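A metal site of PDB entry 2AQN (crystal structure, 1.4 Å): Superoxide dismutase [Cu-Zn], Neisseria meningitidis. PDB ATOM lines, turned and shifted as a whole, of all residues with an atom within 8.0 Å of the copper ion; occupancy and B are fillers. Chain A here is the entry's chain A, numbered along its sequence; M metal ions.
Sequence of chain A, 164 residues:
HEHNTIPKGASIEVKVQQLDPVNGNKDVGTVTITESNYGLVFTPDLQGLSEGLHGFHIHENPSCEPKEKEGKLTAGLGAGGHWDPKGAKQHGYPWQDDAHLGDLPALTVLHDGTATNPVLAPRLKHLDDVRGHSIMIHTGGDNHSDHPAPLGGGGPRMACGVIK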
ATOM      1  N   GLY A  55     -19.652 -13.335   8.348  1.00  0.00           N
ATOM      2  CA  GLY A  55     -18.898 -12.546   9.324  1.00  0.00           C
ATOM      3  C   GLY A  55     -19.865 -11.902  10.335  1.00  0.00           C
ATOM      4  O   GLY A  55     -20.931 -11.415   9.989  1.00  0.00           O
ATOM      5  N   PHE A  56     -19.444 -11.917  11.578  1.00  0.00           N
ATOM      6  CA  PHE A  56     -20.257 -11.528  12.736  1.00  0.00           C
ATOM      7  C   PHE A  56     -19.375 -10.765  13.679  1.00  0.00           C
ATOM      8  O   PHE A  56     -18.429 -11.302  14.262  1.00  0.00           O
ATOM      9  CB  PHE A  56     -20.764 -12.801  13.337  1.00  0.00           C
ATOM     10  CG  PHE A  56     -21.893 -12.819  14.304  1.00  0.00           C
ATOM     11  CD1 PHE A  56     -22.973 -11.962  14.177  1.00  0.00           C
ATOM     12  CD2 PHE A  56     -21.886 -13.700  15.387  1.00  0.00           C
ATOM     13  CE1 PHE A  56     -24.056 -12.034  15.055  1.00  0.00           C
ATOM     14  CE2 PHE A  56     -22.966 -13.806  16.251  1.00  0.00           C
ATOM     15  CZ  PHE A  56     -24.043 -12.944  16.074  1.00  0.00           C
ATOM     16  N   HIS A  57     -19.596  -9.454  13.827  1.00  0.00           N
ATOM     17  CA  HIS A  57     -18.670  -8.627  14.606  1.00  0.00           C
ATOM     18  C   HIS A  57     -19.422  -7.538  15.387  1.00  0.00           C
ATOM     19  O   HIS A  57     -20.465  -7.079  14.931  1.00  0.00           O
ATOM     20  CB  HIS A  57     -17.645  -7.921  13.753  1.00  0.00           C
ATOM     21  CG  HIS A  57     -17.172  -8.631  12.524  1.00  0.00           C
ATOM     22  ND1 HIS A  57     -17.484  -8.212  11.238  1.00  0.00           N
ATOM     23  CD2 HIS A  57     -16.494  -9.806  12.402  1.00  0.00           C
ATOM     24  CE1 HIS A  57     -16.952  -9.080  10.379  1.00  0.00           C
ATOM     25  NE2 HIS A  57     -16.363 -10.039  11.059  1.00  0.00           N
ATOM     26  N   ILE A  58     -18.879  -7.147  16.505  1.00  0.00           N
ATOM     27  CA  ILE A  58     -19.301  -5.896  17.121  1.00  0.00           C
ATOM     28  C   ILE A  58     -18.670  -4.715  16.395  1.00  0.00           C
ATOM     29  O   ILE A  58     -17.445  -4.729  16.272  1.00  0.00           O
ATOM     30  CB  ILE A  58     -18.897  -5.891  18.610  1.00  0.00           C
ATOM     31  CG1 ILE A  58     -19.281  -7.140  19.347  1.00  0.00           C
ATOM     32  CG2 ILE A  58     -19.461  -4.625  19.288  1.00  0.00           C
ATOM     33  CD1 ILE A  58     -20.757  -7.435  19.466  1.00  0.00           C
ATOM     34  N   HIS A  59     -19.490  -3.737  15.998  1.00  0.00           N
ATOM     35  CA  HIS A  59     -19.010  -2.505  15.395  1.00  0.00           C
ATOM     36  C   HIS A  59     -19.119  -1.364  16.404  1.00  0.00           C
ATOM     37  O   HIS A  59     -19.835  -1.426  17.395  1.00  0.00           O
ATOM     38  CB  HIS A  59     -19.734  -2.149  14.080  1.00  0.00           C
ATOM     39  CG  HIS A  59     -19.317  -3.062  12.957  1.00  0.00           C
ATOM     40  ND1 HIS A  59     -18.838  -2.585  11.765  1.00  0.00           N
ATOM     41  CD2 HIS A  59     -19.271  -4.422  12.823  1.00  0.00           C
ATOM     42  CE1 HIS A  59     -18.523  -3.600  10.961  1.00  0.00           C
ATOM     43  NE2 HIS A  59     -18.788  -4.718  11.576  1.00  0.00           N
ATOM     44  N   ALA A  79     -22.595   2.312  11.424  1.00  0.00           N
ATOM     45  CA  ALA A  79     -22.072   1.561  12.558  1.00  0.00           C
ATOM     46  C   ALA A  79     -20.578   1.740  12.787  1.00  0.00           C
ATOM     47  O   ALA A  79     -20.035   1.382  13.811  1.00  0.00           O
ATOM     48  CB  ALA A  79     -22.355   0.067  12.370  1.00  0.00           C
ATOM     49  N   GLY A  80     -19.901   2.334  11.792  1.00  0.00           N
ATOM     50  CA  GLY A  80     -18.455   2.453  11.836  1.00  0.00           C
ATOM     51  C   GLY A  80     -17.741   1.131  11.668  1.00  0.00           C
ATOM     52  O   GLY A  80     -18.293   0.161  11.099  1.00  0.00           O
ATOM     53  N   GLY A  81     -16.496   1.129  12.148  1.00  0.00           N
ATOM     54  CA  GLY A  81     -15.665  -0.057  11.867  1.00  0.00           C
ATOM     55  C   GLY A  81     -15.824  -1.077  12.998  1.00  0.00           C
ATOM     56  O   GLY A  81     -16.643  -0.938  13.918  1.00  0.00           O
ATOM     57  N   HIS A  82     -15.012  -2.146  12.915  1.00  0.00           N
ATOM     58  CA  HIS A  82     -14.966  -3.125  13.982  1.00  0.00           C
ATOM     59  C   HIS A  82     -14.552  -2.462  15.278  1.00  0.00           C
ATOM     60  O   HIS A  82     -13.620  -1.664  15.316  1.00  0.00           O
ATOM     61  CB  HIS A  82     -14.007  -4.289  13.662  1.00  0.00           C
ATOM     62  CG  HIS A  82     -14.412  -5.080  12.459  1.00  0.00           C
ATOM     63  ND1 HIS A  82     -13.851  -6.289  12.220  1.00  0.00           N
ATOM     64  CD2 HIS A  82     -15.299  -4.858  11.462  1.00  0.00           C
ATOM     65  CE1 HIS A  82     -14.387  -6.776  11.092  1.00  0.00           C
ATOM     66  NE2 HIS A  82     -15.283  -5.924  10.606  1.00  0.00           N
ATOM     67  N   TRP A  83     -15.269  -2.845  16.338  1.00  0.00           N
ATOM     68  CA  TRP A  83     -14.964  -2.279  17.665  1.00  0.00           C
ATOM     69  C   TRP A  83     -13.571  -2.670  18.088  1.00  0.00           C
ATOM     70  O   TRP A  83     -13.280  -3.885  18.178  1.00  0.00           O
ATOM     71  CB  TRP A  83     -16.060  -2.680  18.662  1.00  0.00           C
ATOM     72  CG  TRP A  83     -15.903  -2.015  20.009  1.00  0.00           C
ATOM     73  CD1 TRP A  83     -15.667  -0.683  20.243  1.00  0.00           C
ATOM     74  CD2 TRP A  83     -15.972  -2.649  21.271  1.00  0.00           C
ATOM     75  NE1 TRP A  83     -15.582  -0.468  21.597  1.00  0.00           N
ATOM     76  CE2 TRP A  83     -15.772  -1.652  22.254  1.00  0.00           C
ATOM     77  CE3 TRP A  83     -16.181  -3.947  21.686  1.00  0.00           C
ATOM     78  CZ2 TRP A  83     -15.768  -1.892  23.616  1.00  0.00           C
ATOM     79  CZ3 TRP A  83     -16.182  -4.198  23.055  1.00  0.00           C
ATOM     80  CH2 TRP A  83     -15.978  -3.177  23.975  1.00  0.00           C
ATOM     81  N   HIS A  91      -7.775  -7.288  12.041  1.00  0.00           N
ATOM     82  CA  HIS A  91      -8.841  -8.272  12.169  1.00  0.00           C
ATOM     83  C   HIS A  91      -8.273  -9.667  12.427  1.00  0.00           C
ATOM     84  O   HIS A  91      -7.262 -10.052  11.869  1.00  0.00           O
ATOM     85  CB  HIS A  91      -9.686  -8.292  10.890  1.00  0.00           C
ATOM     86  CG  HIS A  91     -10.897  -9.159  11.040  1.00  0.00           C
ATOM     87  ND1 HIS A  91     -11.965  -8.871  11.839  1.00  0.00           N
ATOM     88  CD2 HIS A  91     -11.137 -10.363  10.429  1.00  0.00           C
ATOM     89  CE1 HIS A  91     -12.842  -9.869  11.721  1.00  0.00           C
ATOM     90  NE2 HIS A  91     -12.372 -10.767  10.882  1.00  0.00           N
ATOM     91  N   HIS A 100      -9.104  -7.115  16.815  1.00  0.00           N
ATOM     92  CA  HIS A 100     -10.239  -6.284  17.254  1.00  0.00           C
ATOM     93  C   HIS A 100     -11.063  -6.974  18.344  1.00  0.00           C
ATOM     94  O   HIS A 100     -11.401  -8.159  18.145  1.00  0.00           O
ATOM     95  CB  HIS A 100     -11.164  -6.007  16.098  1.00  0.00           C
ATOM     96  CG  HIS A 100     -10.646  -5.434  14.829  1.00  0.00           C
ATOM     97  ND1 HIS A 100     -11.012  -5.859  13.595  1.00  0.00           N
ATOM     98  CD2 HIS A 100      -9.817  -4.370  14.625  1.00  0.00           C
ATOM     99  CE1 HIS A 100     -10.407  -5.102  12.677  1.00  0.00           C
ATOM    100  NE2 HIS A 100      -9.665  -4.188  13.277  1.00  0.00           N
ATOM    101  N   GLY A 102     -14.088  -6.638  18.923  1.00  0.00           N
ATOM    102  CA  GLY A 102     -15.390  -7.009  18.381  1.00  0.00           C
ATOM    103  C   GLY A 102     -15.390  -8.222  17.495  1.00  0.00           C
ATOM    104  O   GLY A 102     -16.461  -8.523  16.948  1.00  0.00           O
ATOM    105  N   ASP A 103     -14.304  -8.936  17.296  1.00  0.00           N
ATOM    106  CA  ASP A 103     -14.259 -10.093  16.346  1.00  0.00           C
ATOM    107  C   ASP A 103     -14.878 -11.321  16.995  1.00  0.00           C
ATOM    108  O   ASP A 103     -14.308 -11.861  17.947  1.00  0.00           O
ATOM    109  CB  ASP A 103     -12.816 -10.339  15.891  1.00  0.00           C
ATOM    110  CG  ASP A 103     -12.247  -9.193  15.047  1.00  0.00           C
ATOM    111  OD1 ASP A 103     -13.070  -8.325  14.587  1.00  0.00           O
ATOM    112  OD2 ASP A 103     -11.015  -9.139  14.847  1.00  0.00           O
ATOM    113  N   SER A 134     -22.900  -1.925  18.106  1.00  0.00           N
ATOM    114  CA  SER A 134     -23.814  -2.622  17.224  1.00  0.00           C
ATOM    115  C   SER A 134     -23.275  -4.027  16.925  1.00  0.00           C
ATOM    116  O   SER A 134     -22.067  -4.240  17.113  1.00  0.00           O
ATOM    117  CB  SER A 134     -23.954  -1.812  15.925  1.00  0.00           C
ATOM    118  OG  SER A 134     -22.697  -1.391  15.442  1.00  0.00           O
ATOM    119  N   ILE A 135     -24.169  -4.923  16.515  1.00  0.00           N
ATOM    120  CA  ILE A 135     -23.736  -6.240  16.061  1.00  0.00           C
ATOM    121  C   ILE A 135     -24.064  -6.343  14.585  1.00  0.00           C
ATOM    122  O   ILE A 135     -25.177  -6.024  14.145  1.00  0.00           O
ATOM    123  CB  ILE A 135     -24.317  -7.379  16.923  1.00  0.00           C
ATOM    124  CG1 ILE A 135     -23.675  -8.712  16.525  1.00  0.00           C
ATOM    125  CG2 ILE A 135     -25.822  -7.392  16.958  1.00  0.00           C
ATOM    126  CD1 ILE A 135     -23.643  -9.792  17.569  1.00  0.00           C
ATOM    127  N   MET A 136     -23.082  -6.766  13.785  1.00  0.00           N
ATOM    128  CA  MET A 136     -23.177  -6.794  12.348  1.00  0.00           C
ATOM    129  C   MET A 136     -23.071  -8.231  11.820  1.00  0.00           C
ATOM    130  O   MET A 136     -22.254  -9.007  12.282  1.00  0.00           O
ATOM    131  CB  MET A 136     -22.038  -5.963  11.746  1.00  0.00           C
ATOM    132  CG  MET A 136     -22.251  -5.526  10.322  1.00  0.00           C
ATOM    133  SD  MET A 136     -23.530  -4.285  10.150  1.00  0.00           S
ATOM    134  CE  MET A 136     -22.793  -2.921  11.076  1.00  0.00           C
ATOM    135  N   ILE A 137     -23.884  -8.527  10.801  1.00  0.00           N
ATOM    136  CA  ILE A 137     -23.810  -9.755  10.067  1.00  0.00           C
ATOM    137  C   ILE A 137     -23.533  -9.382   8.585  1.00  0.00           C
ATOM    138  O   ILE A 137     -24.264  -8.614   7.976  1.00  0.00           O
ATOM    139  CB  ILE A 137     -25.081 -10.619  10.169  1.00  0.00           C
ATOM    140  CG1 ILE A 137     -25.429 -10.909  11.612  1.00  0.00           C
ATOM    141  CG2 ILE A 137     -24.960 -11.877   9.342  1.00  0.00           C
ATOM    142  CD1 ILE A 137     -26.822 -11.447  11.872  1.00  0.00           C
ATOM    143  N   HIS A 138     -22.429  -9.898   8.076  1.00  0.00           N
ATOM    144  CA  HIS A 138     -21.988  -9.601   6.728  1.00  0.00           C
ATOM    145  C   HIS A 138     -22.514 -10.583   5.694  1.00  0.00           C
ATOM    146  O   HIS A 138     -22.946 -11.691   5.991  1.00  0.00           O
ATOM    147  CB  HIS A 138     -20.441  -9.553   6.714  1.00  0.00           C
ATOM    148  CG  HIS A 138     -19.891  -8.405   7.481  1.00  0.00           C
ATOM    149  ND1 HIS A 138     -19.535  -7.210   6.892  1.00  0.00           N
ATOM    150  CD2 HIS A 138     -19.684  -8.204   8.805  1.00  0.00           C
ATOM    151  CE1 HIS A 138     -19.104  -6.364   7.817  1.00  0.00           C
ATOM    152  NE2 HIS A 138     -19.170  -6.918   9.005  1.00  0.00           N
ATOM    153  N   ASP A 142     -15.899 -15.170   7.096  1.00  0.00           N
ATOM    154  CA  ASP A 142     -14.837 -14.600   7.938  1.00  0.00           C
ATOM    155  C   ASP A 142     -13.686 -15.596   8.079  1.00  0.00           C
ATOM    156  O   ASP A 142     -13.815 -16.603   8.779  1.00  0.00           O
ATOM    157  CB  ASP A 142     -15.362 -14.201   9.304  1.00  0.00           C
ATOM    158  CG  ASP A 142     -14.491 -13.262  10.111  1.00  0.00           C
ATOM    159  OD1 ASP A 142     -13.319 -13.100   9.751  1.00  0.00           O
ATOM    160  OD2 ASP A 142     -14.970 -12.637  11.130  1.00  0.00           O
ATOM    161  N   LEU A 151     -10.752  -7.474   6.701  1.00  0.00           N
ATOM    162  CA  LEU A 151     -11.854  -7.750   7.619  1.00  0.00           C
ATOM    163  C   LEU A 151     -12.504  -9.086   7.368  1.00  0.00           C
ATOM    164  O   LEU A 151     -13.718  -9.275   7.512  1.00  0.00           O
ATOM    165  CB  LEU A 151     -12.849  -6.592   7.545  1.00  0.00           C
ATOM    166  CG  LEU A 151     -12.218  -5.202   7.831  1.00  0.00           C
ATOM    167  CD1 LEU A 151     -13.117  -4.080   7.355  1.00  0.00           C
ATOM    168  CD2 LEU A 151     -11.910  -5.023   9.315  1.00  0.00           C
ATOM    169  N   GLY A 154     -15.695 -10.289   4.966  1.00  0.00           N
ATOM    170  CA  GLY A 154     -17.132 -10.159   5.196  1.00  0.00           C
ATOM    171  C   GLY A 154     -17.772  -9.291   4.159  1.00  0.00           C
ATOM    172  O   GLY A 154     -18.947  -9.503   3.813  1.00  0.00           O
ATOM    173  N   GLY A 155     -17.080  -8.280   3.657  1.00  0.00           N
ATOM    174  CA  GLY A 155     -17.704  -7.447   2.633  1.00  0.00           C
ATOM    175  C   GLY A 155     -18.908  -6.689   3.165  1.00  0.00           C
ATOM    176  O   GLY A 155     -18.904  -6.199   4.312  1.00  0.00           O
ATOM    177  N   PRO A 156     -19.914  -6.535   2.322  1.00  0.00           N
ATOM    178  CA  PRO A 156     -21.108  -5.770   2.650  1.00  0.00           C
ATOM    179  C   PRO A 156     -21.811  -6.189   3.912  1.00  0.00           C
ATOM    180  O   PRO A 156     -21.709  -7.306   4.385  1.00  0.00           O
ATOM    181  CB  PRO A 156     -22.024  -5.971   1.425  1.00  0.00           C
ATOM    182  CG  PRO A 156     -21.105  -6.242   0.305  1.00  0.00           C
ATOM    183  CD  PRO A 156     -19.917  -6.963   0.888  1.00  0.00           C
ATOM    184  N   ARG A 157     -22.539  -5.229   4.493  1.00  0.00           N
ATOM    185  CA  ARG A 157     -23.269  -5.406   5.743  1.00  0.00           C
ATOM    186  C   ARG A 157     -24.692  -5.808   5.391  1.00  0.00           C
ATOM    187  O   ARG A 157     -25.390  -5.020   4.751  1.00  0.00           O
ATOM    188  CB  ARG A 157     -23.202  -4.085   6.549  1.00  0.00           C
ATOM    189  CG  ARG A 157     -21.775  -3.698   6.876  1.00  0.00           C
ATOM    190  CD  ARG A 157     -21.573  -2.295   7.404  1.00  0.00           C
ATOM    191  NE  ARG A 157     -20.142  -2.073   7.513  1.00  0.00           N
ATOM    192  CZ  ARG A 157     -19.537  -1.222   8.343  1.00  0.00           C
ATOM    193  NH1 ARG A 157     -20.262  -0.466   9.193  1.00  0.00           N
ATOM    194  NH2 ARG A 157     -18.212  -1.137   8.329  1.00  0.00           N
ATOM    195  N   ALA A 159     -27.091  -7.459   7.747  1.00  0.00           N
ATOM    196  CA  ALA A 159     -28.055  -7.373   8.842  1.00  0.00           C
ATOM    197  C   ALA A 159     -27.352  -6.770  10.057  1.00  0.00           C
ATOM    198  O   ALA A 159     -26.105  -6.862  10.164  1.00  0.00           O
ATOM    199  CB  ALA A 159     -28.669  -8.735   9.184  1.00  0.00           C
HETATM  200 CU    CU M   1     -18.372  -6.474  10.846  1.00  0.00          CU
HETATM  201 ZN    ZN M   2     -12.341  -7.316  13.117  1.00  0.00          ZN
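The backbone carbonyl oxygen (O) of His 57 is in hydrogen-bond range of the backbone NH (N) of Met 136 (2.9 Å). O of Gly 80 is in hydrogen-bond range of ND1 of His 59 (2.9 Å). NE2 of His 57 lies within hydrogen-bond range of OD2 of Asp 142 (2.9 Å). A ring nitrogen (ND1) of His 57 lies close to a ring nitrogen (NE2) of His 82, 3.2 Å away. A ring nitrogen (ND1) of His 138 lies close to the backbone carbonyl oxygen (O) of Pro 156. The backbone carbonyl oxygen (O) of Ser 134 lies within hydrogen-bond range of the backbone NH (N) of His 59 (2.9 Å). ND1 of His 138 lies within hydrogen-bond range of O of Gly 155. A ring nitrogen (ND1) of His 59 sits close to the backbone carbonyl oxygen of Gly 81 (3.5 Å).
The copper ion is bound by a ring nitrogen (NE2) of His 59, a ring nitrogen (ND1) of His 57 and a ring nitrogen (NE2) of His 138. The copper ion has three donor atoms within binding distance.
Residues that only touch the copper ion: His 82 (3.1 Å) and Met 136 (3.8 Å). Of the 26 residues printed, 5 come within 4 Å of the copper ion.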
